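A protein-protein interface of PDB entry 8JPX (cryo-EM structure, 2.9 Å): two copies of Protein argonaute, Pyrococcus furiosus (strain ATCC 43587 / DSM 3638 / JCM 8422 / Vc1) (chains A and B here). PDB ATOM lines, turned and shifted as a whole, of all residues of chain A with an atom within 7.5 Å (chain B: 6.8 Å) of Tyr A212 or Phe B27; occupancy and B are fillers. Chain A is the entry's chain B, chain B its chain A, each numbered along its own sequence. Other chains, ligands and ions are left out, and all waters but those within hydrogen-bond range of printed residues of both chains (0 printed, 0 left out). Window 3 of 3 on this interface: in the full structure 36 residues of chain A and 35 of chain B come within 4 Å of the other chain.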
ATOM      1  N   ASN A 206      -6.906 -12.426 -10.638  1.00  0.00           N
ATOM      2  CA  ASN A 206      -6.577 -12.599 -12.050  1.00  0.00           C
ATOM      3  C   ASN A 206      -7.803 -12.210 -12.859  1.00  0.00           C
ATOM      4  O   ASN A 206      -8.865 -12.822 -12.701  1.00  0.00           O
ATOM      5  CB  ASN A 206      -6.158 -14.040 -12.346  1.00  0.00           C
ATOM      6  CG  ASN A 206      -5.867 -14.279 -13.816  1.00  0.00           C
ATOM      7  OD1 ASN A 206      -5.727 -13.339 -14.597  1.00  0.00           O
ATOM      8  ND2 ASN A 206      -5.770 -15.546 -14.199  1.00  0.00           N
ATOM      9  N   GLN A 207      -7.657 -11.200 -13.719  1.00  0.00           N
ATOM     10  CA  GLN A 207      -8.801 -10.686 -14.466  1.00  0.00           C
ATOM     11  C   GLN A 207      -9.368 -11.734 -15.416  1.00  0.00           C
ATOM     12  O   GLN A 207     -10.582 -11.781 -15.651  1.00  0.00           O
ATOM     13  CB  GLN A 207      -8.394  -9.429 -15.233  1.00  0.00           C
ATOM     14  CG  GLN A 207      -8.006  -8.259 -14.342  1.00  0.00           C
ATOM     15  CD  GLN A 207      -7.701  -7.001 -15.131  1.00  0.00           C
ATOM     16  OE1 GLN A 207      -8.285  -6.759 -16.187  1.00  0.00           O
ATOM     17  NE2 GLN A 207      -6.782  -6.190 -14.620  1.00  0.00           N
ATOM     18  N   GLU A 208      -8.502 -12.580 -15.978  1.00  0.00           N
ATOM     19  CA  GLU A 208      -8.963 -13.572 -16.943  1.00  0.00           C
ATOM     20  C   GLU A 208      -9.916 -14.573 -16.303  1.00  0.00           C
ATOM     21  O   GLU A 208     -10.922 -14.956 -16.910  1.00  0.00           O
ATOM     22  CB  GLU A 208      -7.767 -14.289 -17.570  1.00  0.00           C
ATOM     23  CG  GLU A 208      -6.564 -13.392 -17.812  1.00  0.00           C
ATOM     24  CD  GLU A 208      -6.839 -12.304 -18.832  1.00  0.00           C
ATOM     25  OE1 GLU A 208      -7.733 -12.491 -19.684  1.00  0.00           O
ATOM     26  OE2 GLU A 208      -6.161 -11.256 -18.782  1.00  0.00           O
ATOM     27  N   ILE A 209      -9.619 -15.002 -15.076  1.00  0.00           N
ATOM     28  CA  ILE A 209     -10.464 -15.987 -14.406  1.00  0.00           C
ATOM     29  C   ILE A 209     -11.847 -15.408 -14.128  1.00  0.00           C
ATOM     30  O   ILE A 209     -12.873 -16.051 -14.390  1.00  0.00           O
ATOM     31  CB  ILE A 209      -9.781 -16.486 -13.120  1.00  0.00           C
ATOM     32  CG1 ILE A 209      -8.888 -17.686 -13.433  1.00  0.00           C
ATOM     33  CG2 ILE A 209     -10.809 -16.859 -12.066  1.00  0.00           C
ATOM     34  CD1 ILE A 209      -7.799 -17.914 -12.420  1.00  0.00           C
ATOM     35  N   VAL A 210     -11.898 -14.182 -13.599  1.00  0.00           N
ATOM     36  CA  VAL A 210     -13.188 -13.576 -13.288  1.00  0.00           C
ATOM     37  C   VAL A 210     -13.977 -13.321 -14.566  1.00  0.00           C
ATOM     38  O   VAL A 210     -15.197 -13.530 -14.609  1.00  0.00           O
ATOM     39  CB  VAL A 210     -12.999 -12.298 -12.443  1.00  0.00           C
ATOM     40  CG1 VAL A 210     -11.980 -12.539 -11.344  1.00  0.00           C
ATOM     41  CG2 VAL A 210     -12.589 -11.106 -13.289  1.00  0.00           C
ATOM     42  N   LYS A 211     -13.295 -12.899 -15.636  1.00  0.00           N
ATOM     43  CA  LYS A 211     -13.975 -12.685 -16.907  1.00  0.00           C
ATOM     44  C   LYS A 211     -14.558 -13.989 -17.434  1.00  0.00           C
ATOM     45  O   LYS A 211     -15.714 -14.035 -17.875  1.00  0.00           O
ATOM     46  CB  LYS A 211     -13.005 -12.079 -17.920  1.00  0.00           C
ATOM     47  CG  LYS A 211     -13.193 -10.592 -18.152  1.00  0.00           C
ATOM     48  CD  LYS A 211     -12.393 -10.121 -19.354  1.00  0.00           C
ATOM     49  CE  LYS A 211     -12.690 -10.964 -20.585  1.00  0.00           C
ATOM     50  NZ  LYS A 211     -14.140 -10.970 -20.922  1.00  0.00           N
ATOM     51  N   TYR A 212     -13.772 -15.067 -17.375  1.00  0.00           N
ATOM     52  CA  TYR A 212     -14.250 -16.352 -17.866  1.00  0.00           C
ATOM     53  C   TYR A 212     -15.451 -16.832 -17.071  1.00  0.00           C
ATOM     54  O   TYR A 212     -16.423 -17.323 -17.650  1.00  0.00           O
ATOM     55  CB  TYR A 212     -13.146 -17.403 -17.804  1.00  0.00           C
ATOM     56  CG  TYR A 212     -13.695 -18.800 -17.976  1.00  0.00           C
ATOM     57  CD1 TYR A 212     -14.237 -19.206 -19.188  1.00  0.00           C
ATOM     58  CD2 TYR A 212     -13.714 -19.697 -16.919  1.00  0.00           C
ATOM     59  CE1 TYR A 212     -14.755 -20.475 -19.349  1.00  0.00           C
ATOM     60  CE2 TYR A 212     -14.234 -20.967 -17.069  1.00  0.00           C
ATOM     61  CZ  TYR A 212     -14.751 -21.351 -18.287  1.00  0.00           C
ATOM     62  OH  TYR A 212     -15.267 -22.617 -18.442  1.00  0.00           O
ATOM     63  N   TRP A 213     -15.403 -16.709 -15.745  1.00  0.00           N
ATOM     64  CA  TRP A 213     -16.509 -17.216 -14.936  1.00  0.00           C
ATOM     65  C   TRP A 213     -17.773 -16.387 -15.135  1.00  0.00           C
ATOM     66  O   TRP A 213     -18.877 -16.940 -15.221  1.00  0.00           O
ATOM     67  CB  TRP A 213     -16.106 -17.263 -13.465  1.00  0.00           C
ATOM     68  CG  TRP A 213     -15.201 -18.412 -13.164  1.00  0.00           C
ATOM     69  CD1 TRP A 213     -13.904 -18.348 -12.754  1.00  0.00           C
ATOM     70  CD2 TRP A 213     -15.519 -19.804 -13.273  1.00  0.00           C
ATOM     71  NE1 TRP A 213     -13.395 -19.612 -12.591  1.00  0.00           N
ATOM     72  CE2 TRP A 213     -14.369 -20.524 -12.902  1.00  0.00           C
ATOM     73  CE3 TRP A 213     -16.667 -20.510 -13.640  1.00  0.00           C
ATOM     74  CZ2 TRP A 213     -14.333 -21.915 -12.890  1.00  0.00           C
ATOM     75  CZ3 TRP A 213     -16.629 -21.889 -13.628  1.00  0.00           C
ATOM     76  CH2 TRP A 213     -15.471 -22.578 -13.255  1.00  0.00           C
ATOM     77  N   TYR A 214     -17.633 -15.062 -15.224  1.00  0.00           N
ATOM     78  CA  TYR A 214     -18.793 -14.212 -15.468  1.00  0.00           C
ATOM     79  C   TYR A 214     -19.426 -14.532 -16.821  1.00  0.00           C
ATOM     80  O   TYR A 214     -20.652 -14.701 -16.923  1.00  0.00           O
ATOM     81  CB  TYR A 214     -18.357 -12.748 -15.376  1.00  0.00           C
ATOM     82  CG  TYR A 214     -19.454 -11.707 -15.404  1.00  0.00           C
ATOM     83  CD1 TYR A 214     -20.175 -11.441 -16.558  1.00  0.00           C
ATOM     84  CD2 TYR A 214     -19.752 -10.973 -14.263  1.00  0.00           C
ATOM     85  CE1 TYR A 214     -21.166 -10.479 -16.570  1.00  0.00           C
ATOM     86  CE2 TYR A 214     -20.743 -10.014 -14.269  1.00  0.00           C
ATOM     87  CZ  TYR A 214     -21.446  -9.771 -15.425  1.00  0.00           C
ATOM     88  OH  TYR A 214     -22.435  -8.815 -15.438  1.00  0.00           O
ATOM     89  N   ASN A 215     -18.602 -14.664 -17.866  1.00  0.00           N
ATOM     90  CA  ASN A 215     -19.141 -14.990 -19.182  1.00  0.00           C
ATOM     91  C   ASN A 215     -19.707 -16.403 -19.227  1.00  0.00           C
ATOM     92  O   ASN A 215     -20.669 -16.657 -19.957  1.00  0.00           O
ATOM     93  CB  ASN A 215     -18.062 -14.810 -20.248  1.00  0.00           C
ATOM     94  CG  ASN A 215     -17.645 -13.364 -20.410  1.00  0.00           C
ATOM     95  OD1 ASN A 215     -18.341 -12.575 -21.048  1.00  0.00           O
ATOM     96  ND2 ASN A 215     -16.506 -13.006 -19.831  1.00  0.00           N
ATOM     97  N   TYR A 216     -19.132 -17.331 -18.461  1.00  0.00           N
ATOM     98  CA  TYR A 216     -19.676 -18.681 -18.377  1.00  0.00           C
ATOM     99  C   TYR A 216     -21.059 -18.669 -17.745  1.00  0.00           C
ATOM    100  O   TYR A 216     -21.972 -19.362 -18.212  1.00  0.00           O
ATOM    101  CB  TYR A 216     -18.717 -19.568 -17.582  1.00  0.00           C
ATOM    102  CG  TYR A 216     -19.332 -20.819 -16.998  1.00  0.00           C
ATOM    103  CD1 TYR A 216     -19.495 -21.959 -17.769  1.00  0.00           C
ATOM    104  CD2 TYR A 216     -19.727 -20.866 -15.670  1.00  0.00           C
ATOM    105  CE1 TYR A 216     -20.047 -23.106 -17.237  1.00  0.00           C
ATOM    106  CE2 TYR A 216     -20.282 -22.009 -15.130  1.00  0.00           C
ATOM    107  CZ  TYR A 216     -20.439 -23.126 -15.919  1.00  0.00           C
ATOM    108  OH  TYR A 216     -20.992 -24.267 -15.386  1.00  0.00           O
ATOM    109  N   HIS A 217     -21.232 -17.882 -16.682  1.00  0.00           N
ATOM    110  CA  HIS A 217     -22.548 -17.755 -16.068  1.00  0.00           C
ATOM    111  C   HIS A 217     -23.550 -17.139 -17.035  1.00  0.00           C
ATOM    112  O   HIS A 217     -24.716 -17.548 -17.072  1.00  0.00           O
ATOM    113  CB  HIS A 217     -22.455 -16.932 -14.785  1.00  0.00           C
ATOM    114  CG  HIS A 217     -22.165 -17.753 -13.567  1.00  0.00           C
ATOM    115  ND1 HIS A 217     -21.398 -17.290 -12.521  1.00  0.00           N
ATOM    116  CD2 HIS A 217     -22.552 -19.004 -13.225  1.00  0.00           C
ATOM    117  CE1 HIS A 217     -21.318 -18.224 -11.591  1.00  0.00           C
ATOM    118  NE2 HIS A 217     -22.010 -19.274 -11.993  1.00  0.00           N
ATOM    119  N   ILE A 218     -23.121 -16.148 -17.821  1.00  0.00           N
ATOM    120  CA  ILE A 218     -24.028 -15.568 -18.812  1.00  0.00           C
ATOM    121  C   ILE A 218     -24.409 -16.601 -19.868  1.00  0.00           C
ATOM    122  O   ILE A 218     -25.589 -16.777 -20.191  1.00  0.00           O
ATOM    123  CB  ILE A 218     -23.410 -14.315 -19.457  1.00  0.00           C
ATOM    124  CG1 ILE A 218     -23.776 -13.065 -18.665  1.00  0.00           C
ATOM    125  CG2 ILE A 218     -23.885 -14.153 -20.892  1.00  0.00           C
ATOM    126  CD1 ILE A 218     -22.939 -11.874 -19.030  1.00  0.00           C
ATOM    127  N   ARG A 220     -24.006 -20.095 -20.165  1.00  0.00           N
ATOM    128  CA  ARG A 220     -24.515 -21.441 -19.919  1.00  0.00           C
ATOM    129  C   ARG A 220     -26.002 -21.435 -19.582  1.00  0.00           C
ATOM    130  O   ARG A 220     -26.752 -22.300 -20.050  1.00  0.00           O
ATOM    131  CB  ARG A 220     -23.714 -22.111 -18.803  1.00  0.00           C
ATOM    132  CG  ARG A 220     -24.318 -23.417 -18.305  1.00  0.00           C
ATOM    133  CD  ARG A 220     -23.682 -24.624 -18.979  1.00  0.00           C
ATOM    134  NE  ARG A 220     -22.238 -24.483 -19.116  1.00  0.00           N
ATOM    135  CZ  ARG A 220     -21.445 -25.385 -19.677  1.00  0.00           C
ATOM    136  NH1 ARG A 220     -21.923 -26.516 -20.168  1.00  0.00           N
ATOM    137  NH2 ARG A 220     -20.138 -25.148 -19.746  1.00  0.00           N
ATOM    138  N   VAL A 238     -19.083  -6.313 -15.565  1.00  0.00           N
ATOM    139  CA  VAL A 238     -18.062  -7.244 -15.103  1.00  0.00           C
ATOM    140  C   VAL A 238     -17.062  -6.480 -14.248  1.00  0.00           C
ATOM    141  O   VAL A 238     -16.084  -5.927 -14.764  1.00  0.00           O
ATOM    142  CB  VAL A 238     -17.356  -7.931 -16.284  1.00  0.00           C
ATOM    143  CG1 VAL A 238     -16.383  -8.986 -15.783  1.00  0.00           C
ATOM    144  CG2 VAL A 238     -18.372  -8.525 -17.229  1.00  0.00           C
ATOM    145  N   TYR A 259     -12.700 -31.183  -7.216  1.00  0.00           N
ATOM    146  CA  TYR A 259     -13.283 -30.174  -8.093  1.00  0.00           C
ATOM    147  C   TYR A 259     -13.288 -28.842  -7.355  1.00  0.00           C
ATOM    148  O   TYR A 259     -14.267 -28.488  -6.694  1.00  0.00           O
ATOM    149  CB  TYR A 259     -14.688 -30.587  -8.516  1.00  0.00           C
ATOM    150  CG  TYR A 259     -15.253 -29.785  -9.664  1.00  0.00           C
ATOM    151  CD1 TYR A 259     -14.419 -29.117 -10.550  1.00  0.00           C
ATOM    152  CD2 TYR A 259     -16.625 -29.694  -9.861  1.00  0.00           C
ATOM    153  CE1 TYR A 259     -14.935 -28.380 -11.599  1.00  0.00           C
ATOM    154  CE2 TYR A 259     -17.150 -28.962 -10.907  1.00  0.00           C
ATOM    155  CZ  TYR A 259     -16.300 -28.307 -11.773  1.00  0.00           C
ATOM    156  OH  TYR A 259     -16.820 -27.577 -12.817  1.00  0.00           O
ATOM    157  N   LYS A 260     -12.187 -28.107  -7.462  1.00  0.00           N
ATOM    158  CA  LYS A 260     -12.138 -26.751  -6.944  1.00  0.00           C
ATOM    159  C   LYS A 260     -13.111 -25.866  -7.720  1.00  0.00           C
ATOM    160  O   LYS A 260     -13.436 -26.128  -8.881  1.00  0.00           O
ATOM    161  CB  LYS A 260     -10.717 -26.194  -7.046  1.00  0.00           C
ATOM    162  CG  LYS A 260     -10.496 -25.272  -8.238  1.00  0.00           C
ATOM    163  CD  LYS A 260      -9.021 -25.059  -8.539  1.00  0.00           C
ATOM    164  CE  LYS A 260      -8.211 -24.839  -7.277  1.00  0.00           C
ATOM    165  NZ  LYS A 260      -6.961 -24.077  -7.543  1.00  0.00           N
ATOM    166  N   ILE A 261     -13.596 -24.817  -7.061  1.00  0.00           N
ATOM    167  CA  ILE A 261     -14.448 -23.852  -7.742  1.00  0.00           C
ATOM    168  C   ILE A 261     -13.980 -22.450  -7.388  1.00  0.00           C
ATOM    169  O   ILE A 261     -13.447 -22.203  -6.301  1.00  0.00           O
ATOM    170  CB  ILE A 261     -15.946 -24.058  -7.409  1.00  0.00           C
ATOM    171  CG1 ILE A 261     -16.809 -23.699  -8.618  1.00  0.00           C
ATOM    172  CG2 ILE A 261     -16.368 -23.216  -6.223  1.00  0.00           C
ATOM    173  CD1 ILE A 261     -16.574 -24.584  -9.820  1.00  0.00           C
ATOM    174  N   TYR A 262     -14.162 -21.536  -8.335  1.00  0.00           N
ATOM    175  CA  TYR A 262     -13.871 -20.124  -8.149  1.00  0.00           C
ATOM    176  C   TYR A 262     -15.189 -19.375  -8.062  1.00  0.00           C
ATOM    177  O   TYR A 262     -16.023 -19.474  -8.968  1.00  0.00           O
ATOM    178  CB  TYR A 262     -13.026 -19.576  -9.302  1.00  0.00           C
ATOM    179  CG  TYR A 262     -11.558 -19.914  -9.209  1.00  0.00           C
ATOM    180  CD1 TYR A 262     -10.681 -19.097  -8.513  1.00  0.00           C
ATOM    181  CD2 TYR A 262     -11.050 -21.051  -9.818  1.00  0.00           C
ATOM    182  CE1 TYR A 262      -9.340 -19.401  -8.427  1.00  0.00           C
ATOM    183  CE2 TYR A 262      -9.711 -21.366  -9.736  1.00  0.00           C
ATOM    184  CZ  TYR A 262      -8.861 -20.537  -9.039  1.00  0.00           C
ATOM    185  OH  TYR A 262      -7.522 -20.845  -8.955  1.00  0.00           O
ATOM    186  N   LEU A 264     -17.068 -15.715  -7.689  1.00  0.00           N
ATOM    187  CA  LEU A 264     -16.962 -14.265  -7.732  1.00  0.00           C
ATOM    188  C   LEU A 264     -17.787 -13.671  -6.603  1.00  0.00           C
ATOM    189  O   LEU A 264     -18.989 -13.947  -6.518  1.00  0.00           O
ATOM    190  CB  LEU A 264     -17.455 -13.726  -9.066  1.00  0.00           C
ATOM    191  CG  LEU A 264     -16.765 -14.289 -10.306  1.00  0.00           C
ATOM    192  CD1 LEU A 264     -17.333 -13.660 -11.565  1.00  0.00           C
ATOM    193  CD2 LEU A 264     -15.268 -14.073 -10.215  1.00  0.00           C
ATOM    194  N   ARG B  25      -2.996 -23.806 -20.015  1.00  0.00           N
ATOM    195  CA  ARG B  25      -3.759 -23.761 -18.778  1.00  0.00           C
ATOM    196  C   ARG B  25      -5.241 -23.788 -19.108  1.00  0.00           C
ATOM    197  O   ARG B  25      -5.719 -22.968 -19.899  1.00  0.00           O
ATOM    198  CB  ARG B  25      -3.426 -22.511 -17.959  1.00  0.00           C
ATOM    199  CG  ARG B  25      -4.538 -22.086 -17.017  1.00  0.00           C
ATOM    200  CD  ARG B  25      -4.078 -21.003 -16.059  1.00  0.00           C
ATOM    201  NE  ARG B  25      -4.533 -21.260 -14.698  1.00  0.00           N
ATOM    202  CZ  ARG B  25      -4.158 -20.557 -13.638  1.00  0.00           C
ATOM    203  NH1 ARG B  25      -3.317 -19.542 -13.744  1.00  0.00           N
ATOM    204  NH2 ARG B  25      -4.639 -20.882 -12.442  1.00  0.00           N
ATOM    205  N   LEU B  26      -5.961 -24.724 -18.503  1.00  0.00           N
ATOM    206  CA  LEU B  26      -7.403 -24.797 -18.667  1.00  0.00           C
ATOM    207  C   LEU B  26      -8.097 -24.006 -17.566  1.00  0.00           C
ATOM    208  O   LEU B  26      -7.505 -23.663 -16.541  1.00  0.00           O
ATOM    209  CB  LEU B  26      -7.891 -26.246 -18.650  1.00  0.00           C
ATOM    210  CG  LEU B  26      -7.277 -27.275 -19.599  1.00  0.00           C
ATOM    211  CD1 LEU B  26      -8.280 -28.381 -19.855  1.00  0.00           C
ATOM    212  CD2 LEU B  26      -6.837 -26.647 -20.907  1.00  0.00           C
ATOM    213  N   PHE B  27      -9.375 -23.719 -17.794  1.00  0.00           N
ATOM    214  CA  PHE B  27     -10.181 -22.985 -16.832  1.00  0.00           C
ATOM    215  C   PHE B  27     -11.157 -23.865 -16.072  1.00  0.00           C
ATOM    216  O   PHE B  27     -11.599 -23.479 -14.985  1.00  0.00           O
ATOM    217  CB  PHE B  27     -10.960 -21.873 -17.539  1.00  0.00           C
ATOM    218  CG  PHE B  27     -10.122 -20.692 -17.916  1.00  0.00           C
ATOM    219  CD1 PHE B  27      -9.214 -20.160 -17.017  1.00  0.00           C
ATOM    220  CD2 PHE B  27     -10.241 -20.111 -19.165  1.00  0.00           C
ATOM    221  CE1 PHE B  27      -8.442 -19.073 -17.357  1.00  0.00           C
ATOM    222  CE2 PHE B  27      -9.470 -19.023 -19.509  1.00  0.00           C
ATOM    223  CZ  PHE B  27      -8.569 -18.503 -18.603  1.00  0.00           C
ATOM    224  N   ASN B  28     -11.501 -25.029 -16.613  1.00  0.00           N
ATOM    225  CA  ASN B  28     -12.499 -25.887 -15.999  1.00  0.00           C
ATOM    226  C   ASN B  28     -12.230 -27.318 -16.438  1.00  0.00           C
ATOM    227  O   ASN B  28     -11.588 -27.560 -17.463  1.00  0.00           O
ATOM    228  CB  ASN B  28     -13.914 -25.428 -16.375  1.00  0.00           C
ATOM    229  CG  ASN B  28     -14.995 -26.321 -15.811  1.00  0.00           C
ATOM    230  OD1 ASN B  28     -15.860 -26.802 -16.541  1.00  0.00           O
ATOM    231  ND2 ASN B  28     -14.955 -26.547 -14.503  1.00  0.00           N
ATOM    232  N   ASP B  29     -12.716 -28.260 -15.639  1.00  0.00           N
ATOM    233  CA  ASP B  29     -12.497 -29.672 -15.911  1.00  0.00           C
ATOM    234  C   ASP B  29     -13.060 -30.029 -17.283  1.00  0.00           C
ATOM    235  O   ASP B  29     -14.227 -29.723 -17.565  1.00  0.00           O
ATOM    236  CB  ASP B  29     -13.170 -30.515 -14.824  1.00  0.00           C
ATOM    237  CG  ASP B  29     -12.777 -31.981 -14.873  1.00  0.00           C
ATOM    238  OD1 ASP B  29     -12.129 -32.409 -15.848  1.00  0.00           O
ATOM    239  OD2 ASP B  29     -13.132 -32.716 -13.928  1.00  0.00           O
ATOM    240  N   GLU B  33     -16.714 -28.727 -19.191  1.00  0.00           N
ATOM    241  CA  GLU B  33     -16.784 -27.841 -20.348  1.00  0.00           C
ATOM    242  C   GLU B  33     -17.450 -28.544 -21.520  1.00  0.00           C
ATOM    243  O   GLU B  33     -18.282 -27.956 -22.219  1.00  0.00           O
ATOM    244  CB  GLU B  33     -15.388 -27.353 -20.731  1.00  0.00           C
ATOM    245  CG  GLU B  33     -14.755 -26.408 -19.726  1.00  0.00           C
ATOM    246  CD  GLU B  33     -13.576 -25.649 -20.306  1.00  0.00           C
ATOM    247  OE1 GLU B  33     -13.799 -24.769 -21.165  1.00  0.00           O
ATOM    248  OE2 GLU B  33     -12.427 -25.927 -19.903  1.00  0.00           O
ATOM    249  N   ASN B  57      -4.376 -26.534 -10.679  1.00  0.00           N
ATOM    250  CA  ASN B  57      -4.599 -25.392 -11.554  1.00  0.00           C
ATOM    251  C   ASN B  57      -4.850 -25.794 -13.000  1.00  0.00           C
ATOM    252  O   ASN B  57      -5.051 -24.913 -13.843  1.00  0.00           O
ATOM    253  CB  ASN B  57      -3.406 -24.435 -11.488  1.00  0.00           C
ATOM    254  CG  ASN B  57      -2.963 -24.160 -10.069  1.00  0.00           C
ATOM    255  OD1 ASN B  57      -3.651 -24.516  -9.114  1.00  0.00           O
ATOM    256  ND2 ASN B  57      -1.807 -23.525  -9.922  1.00  0.00           N
ATOM    257  N   LEU B  58      -4.839 -27.093 -13.302  1.00  0.00           N
ATOM    258  CA  LEU B  58      -5.087 -27.601 -14.651  1.00  0.00           C
ATOM    259  C   LEU B  58      -4.089 -27.024 -15.653  1.00  0.00           C
ATOM    260  O   LEU B  58      -4.460 -26.465 -16.687  1.00  0.00           O
ATOM    261  CB  LEU B  58      -6.527 -27.321 -15.087  1.00  0.00           C
ATOM    262  CG  LEU B  58      -7.630 -27.773 -14.130  1.00  0.00           C
ATOM    263  CD1 LEU B  58      -8.988 -27.325 -14.633  1.00  0.00           C
ATOM    264  CD2 LEU B  58      -7.595 -29.278 -13.951  1.00  0.00           C
ATOM    265  N   GLU B  71     -12.134 -24.036 -23.704  1.00  0.00           N
ATOM    266  CA  GLU B  71     -11.466 -22.781 -23.392  1.00  0.00           C
ATOM    267  C   GLU B  71     -10.146 -23.054 -22.686  1.00  0.00           C
ATOM    268  O   GLU B  71     -10.084 -23.865 -21.756  1.00  0.00           O
ATOM    269  CB  GLU B  71     -12.352 -21.892 -22.516  1.00  0.00           C
ATOM    270  CG  GLU B  71     -13.512 -21.253 -23.258  1.00  0.00           C
ATOM    271  CD  GLU B  71     -13.185 -19.864 -23.764  1.00  0.00           C
ATOM    272  OE1 GLU B  71     -12.036 -19.641 -24.199  1.00  0.00           O
ATOM    273  OE2 GLU B  71     -14.079 -18.992 -23.730  1.00  0.00           O
ATOM    274  N   PHE B  72      -9.094 -22.374 -23.132  1.00  0.00           N
ATOM    275  CA  PHE B  72      -7.768 -22.531 -22.548  1.00  0.00           C
ATOM    276  C   PHE B  72      -6.946 -21.298 -22.888  1.00  0.00           C
ATOM    277  O   PHE B  72      -7.296 -20.520 -23.777  1.00  0.00           O
ATOM    278  CB  PHE B  72      -7.080 -23.799 -23.056  1.00  0.00           C
ATOM    279  CG  PHE B  72      -6.789 -23.785 -24.530  1.00  0.00           C
ATOM    280  CD1 PHE B  72      -7.726 -24.245 -25.438  1.00  0.00           C
ATOM    281  CD2 PHE B  72      -5.575 -23.323 -25.006  1.00  0.00           C
ATOM    282  CE1 PHE B  72      -7.462 -24.234 -26.791  1.00  0.00           C
ATOM    283  CE2 PHE B  72      -5.306 -23.312 -26.359  1.00  0.00           C
ATOM    284  CZ  PHE B  72      -6.250 -23.768 -27.251  1.00  0.00           C
ATOM    285  N   ILE B  73      -5.843 -21.128 -22.166  1.00  0.00           N
ATOM    286  CA  ILE B  73      -4.888 -20.068 -22.488  1.00  0.00           C
ATOM    287  C   ILE B  73      -3.481 -20.649 -22.573  1.00  0.00           C
ATOM    288  O   ILE B  73      -3.090 -21.476 -21.737  1.00  0.00           O
ATOM    289  CB  ILE B  73      -4.963 -18.908 -21.477  1.00  0.00           C
ATOM    290  CG1 ILE B  73      -4.328 -19.285 -20.136  1.00  0.00           C
ATOM    291  CG2 ILE B  73      -6.394 -18.434 -21.298  1.00  0.00           C
ATOM    292  CD1 ILE B  73      -4.554 -18.266 -19.044  1.00  0.00           C
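ND2 of Asn B28 sits at hydrogen-bond distance from OH of Tyr A259 (2.7 Å).
N of Glu B71 lies within hydrogen-bond range of OE1 of Glu B33, 3.1 Å away.
The side-chain amide oxygen (OD1) of Asn B28 lies within hydrogen-bond range of the backbone NH (N) of Glu B33 (3.4 Å).
Among the printed residues, merely in contact across the chains: Tyr A212 with Phe B27 (3.4 Å), Lys A260 with Asn B57 (3.7 Å), Tyr A212 with Asn B28 (3.7 Å), Tyr A212 with Glu B33 (3.8 Å) and Trp A213 with Phe B27 (3.8 Å).
Of the printed residues of chain B, Tyr A212 touches Phe B27 (3.4 Å), Asn B28 (3.7 Å) and Glu B33 (3.8 Å).
Of the printed residues of chain A, Phe B27 touches Tyr A212 (3.4 Å) and Trp A213 (3.8 Å).
Of the printed residues of chain B, Lys A260 touches Asn B57.
Printed residues of chain A within 4 Å of Asn B57: Lys A260 (3.7 Å).
His A217 touches none of the printed residues of chain B.
The nearest residue of chain B that does not touch Tyr A212 is Glu B71 (4.2 Å).
The nearest printed residue of chain A that does not touch Asn B28 is Trp A213 (4.2 Å).
Along chain A the printed residues that touch a printed residue of chain B span positions 212 to 260.
Among the printed residues, 6 pairs touch across the chains.
No position is printed for both chains.
Of the 6 pairs that touch across the chains among the printed residues, none has its exchanged pair printed and touching as well.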
